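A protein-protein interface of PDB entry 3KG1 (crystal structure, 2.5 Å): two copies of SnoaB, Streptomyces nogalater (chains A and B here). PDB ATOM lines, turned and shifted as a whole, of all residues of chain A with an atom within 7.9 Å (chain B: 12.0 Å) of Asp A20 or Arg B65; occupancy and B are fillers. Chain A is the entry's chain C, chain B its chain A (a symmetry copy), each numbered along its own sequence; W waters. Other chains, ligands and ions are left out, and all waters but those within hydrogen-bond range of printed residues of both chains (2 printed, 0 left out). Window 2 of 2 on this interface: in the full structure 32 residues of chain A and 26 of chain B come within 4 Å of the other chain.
The backbone NH (N) of Asp A20 sits close to the guanidinium group (NH1) of Arg B65.
O of Thr A111 is in hydrogen-bond range of N of Arg B63, at 2.8 Å.
O of Asp A22 lies within hydrogen-bond range of NH2 of Arg B65 (3.0 Å).
The backbone carbonyl oxygen (O) of Leu A109 sits at hydrogen-bond distance from the backbone NH (N) of Arg B65 (2.9 Å).
OG1 of Thr A111 sits at hydrogen-bond distance from NE of Arg B65, at 3.2 Å.
The backbone NH (N) of Leu B62 is in hydrogen-bond range of the backbone carbonyl oxygen (O) of Val B72 (2.7 Å).
O of Val A24 lies within hydrogen-bond range of N of Trp A77 (2.8 Å).
NE of Arg B63 lies within hydrogen-bond range of OH of Tyr B71 (3.3 Å).
The backbone carbonyl oxygen of Phe A110 lies within hydrogen-bond range of the backbone NH of Thr A25, at 2.8 Å.
The side-chain hydroxyl (OG) of Ser B70 sits at hydrogen-bond distance from the side-chain carboxylate (OE1) of Glu B64 (2.9 Å).
The backbone carbonyl oxygen (O) of Asp B68 sits at hydrogen-bond distance from the guanidinium group (NH2) of Arg B63.
Arg B65 touches Glu A23 (NH2 to O, 3.7 Å).
Thr A25 touches Leu B62.
Arg B65 touches His A80.
Glu B64 touches Gly A108 (OE2 to CA, 3.6 Å).
Glu B64 touches Leu A109 (CA to O, 3.5 Å).
CB of Leu B62 touches CB of Phe A110 (3.8 Å).
Phe A110 touches Glu B64 (CD2 to N, 3.3 Å).
Thr A111 touches Leu B62.
Ala A112 touches Leu B61.
Ala A112 touches Leu B62 (CA to CD2, 3.8 Å).
No residue of chain B comes within 4 Å of Ala A21.
No residue of chain B comes within 4 Å of Asp A79.
His A80 touches one residue of chain B.
Leu A109 touches two residues of chain B.
Thr A111 touches just these residues of chain B: Leu B62 (3.5 Å), Arg B63 (2.8 Å) and Arg B65 (3.2 Å).
Of the printed residues of chain A, Leu B61 touches Ala A112.
Printed residues of chain A within 4 Å of Arg B63: Phe A110 and Thr A111.
Of the printed residues of chain A, Glu B64 touches Gly A108 (3.6 Å), Leu A109 (3.5 Å) and Phe A110 (3.3 Å).
Printed residues of chain A within 4 Å of Arg B65: Asp A20 (3.2 Å), Asp A22 (3.0 Å), Glu A23 (3.7 Å), Val A24 (3.5 Å), His A80 (3.8 Å), Leu A109 (2.9 Å), Phe A110 (3.99 Å) and Thr A111 (3.2 Å).
Asn B69 touches none of the printed residues of chain A.
The nearest residue of chain B that does not touch Asp A20 is Asp B66 (10.0 Å).
The nearest printed residue of chain A that does not touch Arg B65 is Asp A79 (5.1 Å).
Hydrophobic or aromatic side chains of chain A within 4 Å of the printed part of chain B: Val A24, His A80, Phe A110 and Ala A112.
Along chain A the printed residues that touch a printed residue of chain B span positions 20 to 112.
Of the 15 printed residues of chain B, 6 touch a printed residue of chain A.
Among the printed residues, 19 pairs touch across the chains.
Among the printed residues, no Asp or Glu carboxylate lies within 4 Å of a Lys or Arg side-chain nitrogen of the other chain.
No position is printed for both chains.
Of the 19 pairs that touch across the chains among the printed residues, none has its exchanged pair printed and touching as well.
Water W1 bridges OE2 of Glu B64 (2.5 Å) and N of Leu A109 (2.7 Å).
Water W2 lies within hydrogen-bond range of the backbone carbonyl oxygen (O) of Asp A22 (2.6 Å), the backbone carbonyl oxygen (O) of Asp A20 (2.7 Å), the guanidinium group (NH2) of Arg B65 (2.8 Å) and the backbone NH (N) of His A80 (2.9 Å).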
ATOM      1  N   ASP A  20      10.667 -18.511  18.410  1.00  0.00           N
ATOM      2  CA  ASP A  20      10.570 -19.324  17.170  1.00  0.00           C
ATOM      3  C   ASP A  20      11.408 -20.608  17.321  1.00  0.00           C
ATOM      4  O   ASP A  20      11.568 -21.110  18.442  1.00  0.00           O
ATOM      5  CB  ASP A  20      11.027 -18.483  15.977  1.00  0.00           C
ATOM      6  CG  ASP A  20      10.520 -19.032  14.665  1.00  0.00           C
ATOM      7  OD1 ASP A  20       9.507 -18.505  14.147  1.00  0.00           O
ATOM      8  OD2 ASP A  20      11.113 -20.029  14.180  1.00  0.00           O
ATOM      9  N   ALA A  21      11.932 -21.135  16.208  1.00  0.00           N
ATOM     10  CA  ALA A  21      12.884 -22.273  16.222  1.00  0.00           C
ATOM     11  C   ALA A  21      14.337 -21.853  16.474  1.00  0.00           C
ATOM     12  O   ALA A  21      15.211 -22.702  16.607  1.00  0.00           O
ATOM     13  CB  ALA A  21      12.806 -23.043  14.919  1.00  0.00           C
ATOM     14  N   ASP A  22      14.580 -20.547  16.547  1.00  0.00           N
ATOM     15  CA  ASP A  22      15.938 -20.002  16.639  1.00  0.00           C
ATOM     16  C   ASP A  22      16.657 -20.345  17.956  1.00  0.00           C
ATOM     17  O   ASP A  22      16.046 -20.471  19.006  1.00  0.00           O
ATOM     18  CB  ASP A  22      15.902 -18.480  16.455  1.00  0.00           C
ATOM     19  CG  ASP A  22      15.824 -18.059  15.001  1.00  0.00           C
ATOM     20  OD1 ASP A  22      16.302 -18.805  14.105  1.00  0.00           O
ATOM     21  OD2 ASP A  22      15.287 -16.951  14.753  1.00  0.00           O
ATOM     22  N   GLU A  23      17.966 -20.495  17.871  1.00  0.00           N
ATOM     23  CA  GLU A  23      18.799 -20.658  19.045  1.00  0.00           C
ATOM     24  C   GLU A  23      18.693 -19.381  19.904  1.00  0.00           C
ATOM     25  O   GLU A  23      18.736 -18.270  19.375  1.00  0.00           O
ATOM     26  CB  GLU A  23      20.233 -20.973  18.606  1.00  0.00           C
ATOM     27  CG  GLU A  23      21.326 -20.872  19.673  1.00  0.00           C
ATOM     28  CD  GLU A  23      22.562 -21.677  19.295  1.00  0.00           C
ATOM     29  OE1 GLU A  23      23.644 -21.076  19.162  1.00  0.00           O
ATOM     30  OE2 GLU A  23      22.431 -22.914  19.100  1.00  0.00           O
ATOM     31  N   VAL A  24      18.479 -19.561  21.209  1.00  0.00           N
ATOM     32  CA  VAL A  24      18.285 -18.443  22.129  1.00  0.00           C
ATOM     33  C   VAL A  24      19.488 -18.305  23.048  1.00  0.00           C
ATOM     34  O   VAL A  24      20.043 -19.310  23.551  1.00  0.00           O
ATOM     35  CB  VAL A  24      16.944 -18.537  22.975  1.00  0.00           C
ATOM     36  CG1 VAL A  24      16.970 -19.645  23.989  1.00  0.00           C
ATOM     37  CG2 VAL A  24      16.660 -17.216  23.687  1.00  0.00           C
ATOM     38  N   THR A  25      19.909 -17.054  23.236  1.00  0.00           N
ATOM     39  CA  THR A  25      20.985 -16.725  24.172  1.00  0.00           C
ATOM     40  C   THR A  25      20.417 -15.814  25.239  1.00  0.00           C
ATOM     41  O   THR A  25      20.119 -14.671  24.972  1.00  0.00           O
ATOM     42  CB  THR A  25      22.165 -16.058  23.470  1.00  0.00           C
ATOM     43  OG1 THR A  25      22.659 -16.942  22.456  1.00  0.00           O
ATOM     44  CG2 THR A  25      23.282 -15.713  24.473  1.00  0.00           C
ATOM     45  N   TRP A  77      20.548 -21.912  24.591  1.00  0.00           N
ATOM     46  CA  TRP A  77      19.571 -22.977  24.527  1.00  0.00           C
ATOM     47  C   TRP A  77      19.184 -23.181  23.079  1.00  0.00           C
ATOM     48  O   TRP A  77      19.160 -22.226  22.315  1.00  0.00           O
ATOM     49  CB  TRP A  77      18.350 -22.613  25.386  1.00  0.00           C
ATOM     50  CG  TRP A  77      18.713 -22.468  26.816  1.00  0.00           C
ATOM     51  CD1 TRP A  77      19.186 -21.352  27.429  1.00  0.00           C
ATOM     52  CD2 TRP A  77      18.660 -23.486  27.818  1.00  0.00           C
ATOM     53  NE1 TRP A  77      19.415 -21.596  28.756  1.00  0.00           N
ATOM     54  CE2 TRP A  77      19.112 -22.907  29.023  1.00  0.00           C
ATOM     55  CE3 TRP A  77      18.257 -24.836  27.822  1.00  0.00           C
ATOM     56  CZ2 TRP A  77      19.185 -23.624  30.220  1.00  0.00           C
ATOM     57  CZ3 TRP A  77      18.323 -25.548  29.018  1.00  0.00           C
ATOM     58  CH2 TRP A  77      18.791 -24.934  30.202  1.00  0.00           C
ATOM     59  N   THR A  78      18.877 -24.416  22.691  1.00  0.00           N
ATOM     60  CA  THR A  78      18.589 -24.708  21.266  1.00  0.00           C
ATOM     61  C   THR A  78      17.351 -23.956  20.731  1.00  0.00           C
ATOM     62  O   THR A  78      17.293 -23.621  19.566  1.00  0.00           O
ATOM     63  CB  THR A  78      18.501 -26.227  20.981  1.00  0.00           C
ATOM     64  OG1 THR A  78      17.552 -26.838  21.861  1.00  0.00           O
ATOM     65  CG2 THR A  78      19.870 -26.874  21.163  1.00  0.00           C
ATOM     66  N   ASP A  79      16.379 -23.696  21.600  1.00  0.00           N
ATOM     67  CA  ASP A  79      15.265 -22.791  21.293  1.00  0.00           C
ATOM     68  C   ASP A  79      14.592 -22.233  22.553  1.00  0.00           C
ATOM     69  O   ASP A  79      14.929 -22.614  23.678  1.00  0.00           O
ATOM     70  CB  ASP A  79      14.256 -23.414  20.312  1.00  0.00           C
ATOM     71  CG  ASP A  79      13.556 -24.648  20.843  1.00  0.00           C
ATOM     72  OD1 ASP A  79      12.661 -25.115  20.111  1.00  0.00           O
ATOM     73  OD2 ASP A  79      13.868 -25.169  21.931  1.00  0.00           O
ATOM     74  N   HIS A  80      13.670 -21.298  22.336  1.00  0.00           N
ATOM     75  CA  HIS A  80      12.966 -20.579  23.418  1.00  0.00           C
ATOM     76  C   HIS A  80      12.193 -21.503  24.369  1.00  0.00           C
ATOM     77  O   HIS A  80      12.226 -21.322  25.594  1.00  0.00           O
ATOM     78  CB  HIS A  80      12.028 -19.536  22.799  1.00  0.00           C
ATOM     79  CG  HIS A  80      11.168 -18.818  23.786  1.00  0.00           C
ATOM     80  ND1 HIS A  80      11.677 -18.093  24.847  1.00  0.00           N
ATOM     81  CD2 HIS A  80       9.820 -18.707  23.864  1.00  0.00           C
ATOM     82  CE1 HIS A  80      10.677 -17.566  25.537  1.00  0.00           C
ATOM     83  NE2 HIS A  80       9.541 -17.923  24.960  1.00  0.00           N
ATOM     84  N   ASP A  81      11.506 -22.493  23.797  1.00  0.00           N
ATOM     85  CA  ASP A  81      10.761 -23.493  24.578  1.00  0.00           C
ATOM     86  C   ASP A  81      11.588 -24.369  25.518  1.00  0.00           C
ATOM     87  O   ASP A  81      11.123 -24.651  26.618  1.00  0.00           O
ATOM     88  CB  ASP A  81       9.962 -24.393  23.640  1.00  0.00           C
ATOM     89  CG  ASP A  81       8.821 -23.666  22.987  1.00  0.00           C
ATOM     90  OD1 ASP A  81       8.290 -22.712  23.619  1.00  0.00           O
ATOM     91  OD2 ASP A  81       8.459 -24.072  21.861  1.00  0.00           O
ATOM     92  N   ALA A  82      12.775 -24.820  25.082  1.00  0.00           N
ATOM     93  CA  ALA A  82      13.684 -25.621  25.933  1.00  0.00           C
ATOM     94  C   ALA A  82      14.132 -24.787  27.128  1.00  0.00           C
ATOM     95  O   ALA A  82      14.194 -25.272  28.264  1.00  0.00           O
ATOM     96  CB  ALA A  82      14.894 -26.096  25.146  1.00  0.00           C
ATOM     97  N   GLY A 108      17.561 -10.318  29.381  1.00  0.00           N
ATOM     98  CA  GLY A 108      16.985 -10.187  28.067  1.00  0.00           C
ATOM     99  C   GLY A 108      17.137 -11.501  27.347  1.00  0.00           C
ATOM    100  O   GLY A 108      17.994 -12.317  27.709  1.00  0.00           O
ATOM    101  N   LEU A 109      16.305 -11.707  26.338  1.00  0.00           N
ATOM    102  CA  LEU A 109      16.303 -12.928  25.559  1.00  0.00           C
ATOM    103  C   LEU A 109      16.793 -12.534  24.176  1.00  0.00           C
ATOM    104  O   LEU A 109      16.190 -11.655  23.558  1.00  0.00           O
ATOM    105  CB  LEU A 109      14.890 -13.481  25.459  1.00  0.00           C
ATOM    106  CG  LEU A 109      14.657 -14.914  25.914  1.00  0.00           C
ATOM    107  CD1 LEU A 109      14.803 -14.957  27.410  1.00  0.00           C
ATOM    108  CD2 LEU A 109      13.282 -15.429  25.515  1.00  0.00           C
ATOM    109  N   PHE A 110      17.871 -13.173  23.702  1.00  0.00           N
ATOM    110  CA  PHE A 110      18.484 -12.795  22.422  1.00  0.00           C
ATOM    111  C   PHE A 110      18.605 -13.944  21.432  1.00  0.00           C
ATOM    112  O   PHE A 110      18.480 -15.104  21.785  1.00  0.00           O
ATOM    113  CB  PHE A 110      19.881 -12.211  22.630  1.00  0.00           C
ATOM    114  CG  PHE A 110      19.919 -10.959  23.451  1.00  0.00           C
ATOM    115  CD1 PHE A 110      19.834 -11.019  24.844  1.00  0.00           C
ATOM    116  CD2 PHE A 110      20.080  -9.733  22.845  1.00  0.00           C
ATOM    117  CE1 PHE A 110      19.885  -9.894  25.595  1.00  0.00           C
ATOM    118  CE2 PHE A 110      20.150  -8.576  23.608  1.00  0.00           C
ATOM    119  CZ  PHE A 110      20.055  -8.661  24.985  1.00  0.00           C
ATOM    120  N   THR A 111      18.882 -13.578  20.188  1.00  0.00           N
ATOM    121  CA  THR A 111      19.173 -14.517  19.109  1.00  0.00           C
ATOM    122  C   THR A 111      20.489 -14.082  18.484  1.00  0.00           C
ATOM    123  O   THR A 111      20.679 -12.903  18.237  1.00  0.00           O
ATOM    124  CB  THR A 111      18.081 -14.487  18.027  1.00  0.00           C
ATOM    125  OG1 THR A 111      16.822 -14.830  18.618  1.00  0.00           O
ATOM    126  CG2 THR A 111      18.400 -15.452  16.900  1.00  0.00           C
ATOM    127  N   ALA A 112      21.389 -15.031  18.243  1.00  0.00           N
ATOM    128  CA  ALA A 112      22.692 -14.743  17.632  1.00  0.00           C
ATOM    129  C   ALA A 112      22.551 -14.476  16.134  1.00  0.00           C
ATOM    130  O   ALA A 112      21.952 -15.289  15.430  1.00  0.00           O
ATOM    131  CB  ALA A 112      23.675 -15.889  17.880  1.00  0.00           C
ATOM    132  N   PHE B  30      24.421  -2.280  22.620  1.00  0.00           N
ATOM    133  CA  PHE B  30      24.079  -1.222  21.650  1.00  0.00           C
ATOM    134  C   PHE B  30      22.590  -0.914  21.654  1.00  0.00           C
ATOM    135  O   PHE B  30      21.792  -1.826  21.524  1.00  0.00           O
ATOM    136  CB  PHE B  30      24.478  -1.634  20.229  1.00  0.00           C
ATOM    137  CG  PHE B  30      25.956  -1.724  20.013  1.00  0.00           C
ATOM    138  CD1 PHE B  30      26.600  -2.961  20.014  1.00  0.00           C
ATOM    139  CD2 PHE B  30      26.714  -0.578  19.826  1.00  0.00           C
ATOM    140  CE1 PHE B  30      27.999  -3.057  19.838  1.00  0.00           C
ATOM    141  CE2 PHE B  30      28.115  -0.656  19.644  1.00  0.00           C
ATOM    142  CZ  PHE B  30      28.758  -1.911  19.653  1.00  0.00           C
ATOM    143  N   PRO B  36      18.296  -0.951  11.519  1.00  0.00           N
ATOM    144  CA  PRO B  36      19.076  -2.091  11.984  1.00  0.00           C
ATOM    145  C   PRO B  36      19.967  -2.699  10.902  1.00  0.00           C
ATOM    146  O   PRO B  36      21.083  -3.118  11.197  1.00  0.00           O
ATOM    147  CB  PRO B  36      17.998  -3.086  12.413  1.00  0.00           C
ATOM    148  CG  PRO B  36      16.849  -2.239  12.776  1.00  0.00           C
ATOM    149  CD  PRO B  36      16.865  -1.142  11.773  1.00  0.00           C
ATOM    150  N   GLU B  40      24.024  -3.397  11.372  1.00  0.00           N
ATOM    151  CA  GLU B  40      24.647  -4.721  11.198  1.00  0.00           C
ATOM    152  C   GLU B  40      25.738  -4.723  10.129  1.00  0.00           C
ATOM    153  O   GLU B  40      26.701  -5.470  10.216  1.00  0.00           O
ATOM    154  CB  GLU B  40      23.604  -5.780  10.860  1.00  0.00           C
ATOM    155  CG  GLU B  40      22.886  -6.338  12.072  1.00  0.00           C
ATOM    156  CD  GLU B  40      21.840  -7.415  11.763  1.00  0.00           C
ATOM    157  OE1 GLU B  40      21.089  -7.764  12.692  1.00  0.00           O
ATOM    158  OE2 GLU B  40      21.734  -7.910  10.616  1.00  0.00           O
ATOM    159  N   LEU B  61      27.399 -11.441  17.778  1.00  0.00           N
ATOM    160  CA  LEU B  61      26.395 -10.384  17.801  1.00  0.00           C
ATOM    161  C   LEU B  61      25.047 -10.995  18.153  1.00  0.00           C
ATOM    162  O   LEU B  61      24.631 -11.964  17.541  1.00  0.00           O
ATOM    163  CB  LEU B  61      26.275  -9.679  16.448  1.00  0.00           C
ATOM    164  CG  LEU B  61      25.363  -8.435  16.436  1.00  0.00           C
ATOM    165  CD1 LEU B  61      25.917  -7.364  17.362  1.00  0.00           C
ATOM    166  CD2 LEU B  61      25.182  -7.875  15.039  1.00  0.00           C
ATOM    167  N   LEU B  62      24.369 -10.392  19.128  1.00  0.00           N
ATOM    168  CA  LEU B  62      23.094 -10.850  19.639  1.00  0.00           C
ATOM    169  C   LEU B  62      22.028  -9.776  19.412  1.00  0.00           C
ATOM    170  O   LEU B  62      22.278  -8.590  19.590  1.00  0.00           O
ATOM    171  CB  LEU B  62      23.235 -11.128  21.147  1.00  0.00           C
ATOM    172  CG  LEU B  62      24.260 -12.200  21.594  1.00  0.00           C
ATOM    173  CD1 LEU B  62      24.334 -12.311  23.112  1.00  0.00           C
ATOM    174  CD2 LEU B  62      23.942 -13.559  20.994  1.00  0.00           C
ATOM    175  N   ARG B  63      20.823 -10.194  19.042  1.00  0.00           N
ATOM    176  CA  ARG B  63      19.710  -9.268  18.925  1.00  0.00           C
ATOM    177  C   ARG B  63      18.534  -9.602  19.855  1.00  0.00           C
ATOM    178  O   ARG B  63      18.094 -10.736  19.912  1.00  0.00           O
ATOM    179  CB  ARG B  63      19.243  -9.270  17.493  1.00  0.00           C
ATOM    180  CG  ARG B  63      18.380  -8.099  17.173  1.00  0.00           C
ATOM    181  CD  ARG B  63      17.763  -8.311  15.849  1.00  0.00           C
ATOM    182  NE  ARG B  63      17.132  -7.100  15.360  1.00  0.00           N
ATOM    183  CZ  ARG B  63      16.185  -7.081  14.435  1.00  0.00           C
ATOM    184  NH1 ARG B  63      15.738  -8.221  13.879  1.00  0.00           N
ATOM    185  NH2 ARG B  63      15.682  -5.908  14.076  1.00  0.00           N
ATOM    186  N   GLU B  64      18.013  -8.625  20.580  1.00  0.00           N
ATOM    187  CA  GLU B  64      16.984  -8.924  21.566  1.00  0.00           C
ATOM    188  C   GLU B  64      15.671  -9.266  20.859  1.00  0.00           C
ATOM    189  O   GLU B  64      15.284  -8.606  19.909  1.00  0.00           O
ATOM    190  CB  GLU B  64      16.793  -7.784  22.572  1.00  0.00           C
ATOM    191  CG  GLU B  64      15.943  -8.194  23.805  1.00  0.00           C
ATOM    192  CD  GLU B  64      16.066  -7.253  25.008  1.00  0.00           C
ATOM    193  OE1 GLU B  64      16.787  -6.212  24.911  1.00  0.00           O
ATOM    194  OE2 GLU B  64      15.441  -7.573  26.053  1.00  0.00           O
ATOM    195  N   ARG B  65      15.012 -10.308  21.331  1.00  0.00           N
ATOM    196  CA  ARG B  65      13.861 -10.870  20.662  1.00  0.00           C
ATOM    197  C   ARG B  65      12.638  -9.976  20.647  1.00  0.00           C
ATOM    198  O   ARG B  65      11.929  -9.918  19.643  1.00  0.00           O
ATOM    199  CB  ARG B  65      13.473 -12.177  21.324  1.00  0.00           C
ATOM    200  CG  ARG B  65      14.475 -13.274  21.098  1.00  0.00           C
ATOM    201  CD  ARG B  65      13.760 -14.569  21.130  1.00  0.00           C
ATOM    202  NE  ARG B  65      14.655 -15.657  20.807  1.00  0.00           N
ATOM    203  CZ  ARG B  65      14.268 -16.839  20.347  1.00  0.00           C
ATOM    204  NH1 ARG B  65      12.981 -17.093  20.115  1.00  0.00           N
ATOM    205  NH2 ARG B  65      15.193 -17.763  20.102  1.00  0.00           N
ATOM    206  N   ASP B  66      12.387  -9.273  21.745  1.00  0.00           N
ATOM    207  CA  ASP B  66      11.170  -8.455  21.840  1.00  0.00           C
ATOM    208  C   ASP B  66      11.415  -6.975  21.475  1.00  0.00           C
ATOM    209  O   ASP B  66      10.566  -6.115  21.741  1.00  0.00           O
ATOM    210  CB  ASP B  66      10.536  -8.616  23.234  1.00  0.00           C
ATOM    211  N   LYS B  67      12.541  -6.701  20.829  1.00  0.00           N
ATOM    212  CA  LYS B  67      12.864  -5.357  20.410  1.00  0.00           C
ATOM    213  C   LYS B  67      13.354  -5.413  18.974  1.00  0.00           C
ATOM    214  O   LYS B  67      13.644  -6.486  18.440  1.00  0.00           O
ATOM    215  CB  LYS B  67      13.909  -4.762  21.355  1.00  0.00           C
ATOM    216  CG  LYS B  67      13.350  -4.464  22.746  1.00  0.00           C
ATOM    217  CD  LYS B  67      14.394  -3.895  23.704  1.00  0.00           C
ATOM    218  CE  LYS B  67      13.751  -3.016  24.784  1.00  0.00           C
ATOM    219  NZ  LYS B  67      14.401  -3.163  26.131  1.00  0.00           N
ATOM    220  N   ASP B  68      13.373  -4.259  18.324  1.00  0.00           N
ATOM    221  CA  ASP B  68      14.048  -4.133  17.042  1.00  0.00           C
ATOM    222  C   ASP B  68      15.464  -3.606  17.295  1.00  0.00           C
ATOM    223  O   ASP B  68      16.421  -3.977  16.595  1.00  0.00           O
ATOM    224  N   ASN B  69      15.597  -2.782  18.331  1.00  0.00           N
ATOM    225  CA  ASN B  69      16.766  -1.916  18.491  1.00  0.00           C
ATOM    226  C   ASN B  69      17.734  -2.222  19.633  1.00  0.00           C
ATOM    227  O   ASN B  69      18.559  -1.377  19.953  1.00  0.00           O
ATOM    228  CB  ASN B  69      16.269  -0.467  18.626  1.00  0.00           C
ATOM    229  CG  ASN B  69      15.672  -0.171  19.995  1.00  0.00           C
ATOM    230  OD1 ASN B  69      15.108  -1.054  20.657  1.00  0.00           O
ATOM    231  ND2 ASN B  69      15.815   1.074  20.437  1.00  0.00           N
ATOM    232  N   SER B  70      17.642  -3.389  20.263  1.00  0.00           N
ATOM    233  CA  SER B  70      18.616  -3.771  21.305  1.00  0.00           C
ATOM    234  C   SER B  70      19.555  -4.837  20.786  1.00  0.00           C
ATOM    235  O   SER B  70      19.101  -5.835  20.246  1.00  0.00           O
ATOM    236  CB  SER B  70      17.941  -4.271  22.579  1.00  0.00           C
ATOM    237  OG  SER B  70      18.919  -4.712  23.543  1.00  0.00           O
ATOM    238  N   TYR B  71      20.859  -4.609  20.974  1.00  0.00           N
ATOM    239  CA  TYR B  71      21.901  -5.537  20.556  1.00  0.00           C
ATOM    240  C   TYR B  71      22.994  -5.682  21.645  1.00  0.00           C
ATOM    241  O   TYR B  71      23.205  -4.799  22.476  1.00  0.00           O
ATOM    242  CB  TYR B  71      22.578  -5.051  19.265  1.00  0.00           C
ATOM    243  CG  TYR B  71      21.896  -5.369  17.953  1.00  0.00           C
ATOM    244  CD1 TYR B  71      20.945  -4.516  17.420  1.00  0.00           C
ATOM    245  CD2 TYR B  71      22.275  -6.482  17.193  1.00  0.00           C
ATOM    246  CE1 TYR B  71      20.351  -4.774  16.215  1.00  0.00           C
ATOM    247  CE2 TYR B  71      21.663  -6.750  15.962  1.00  0.00           C
ATOM    248  CZ  TYR B  71      20.706  -5.884  15.489  1.00  0.00           C
ATOM    249  OH  TYR B  71      20.097  -6.114  14.279  1.00  0.00           O
ATOM    250  N   VAL B  72      23.697  -6.805  21.598  1.00  0.00           N
ATOM    251  CA  VAL B  72      24.814  -7.072  22.484  1.00  0.00           C
ATOM    252  C   VAL B  72      25.879  -7.755  21.636  1.00  0.00           C
ATOM    253  O   VAL B  72      25.574  -8.706  20.921  1.00  0.00           O
ATOM    254  CB  VAL B  72      24.422  -7.977  23.702  1.00  0.00           C
ATOM    255  CG1 VAL B  72      25.662  -8.343  24.533  1.00  0.00           C
ATOM    256  CG2 VAL B  72      23.400  -7.299  24.577  1.00  0.00           C
HETATM  257  O   HOH W   1      14.351  -9.855  26.283  1.00  0.00           O
HETATM  258  O   HOH W   2      13.629 -20.044  19.770  1.00  0.00           O
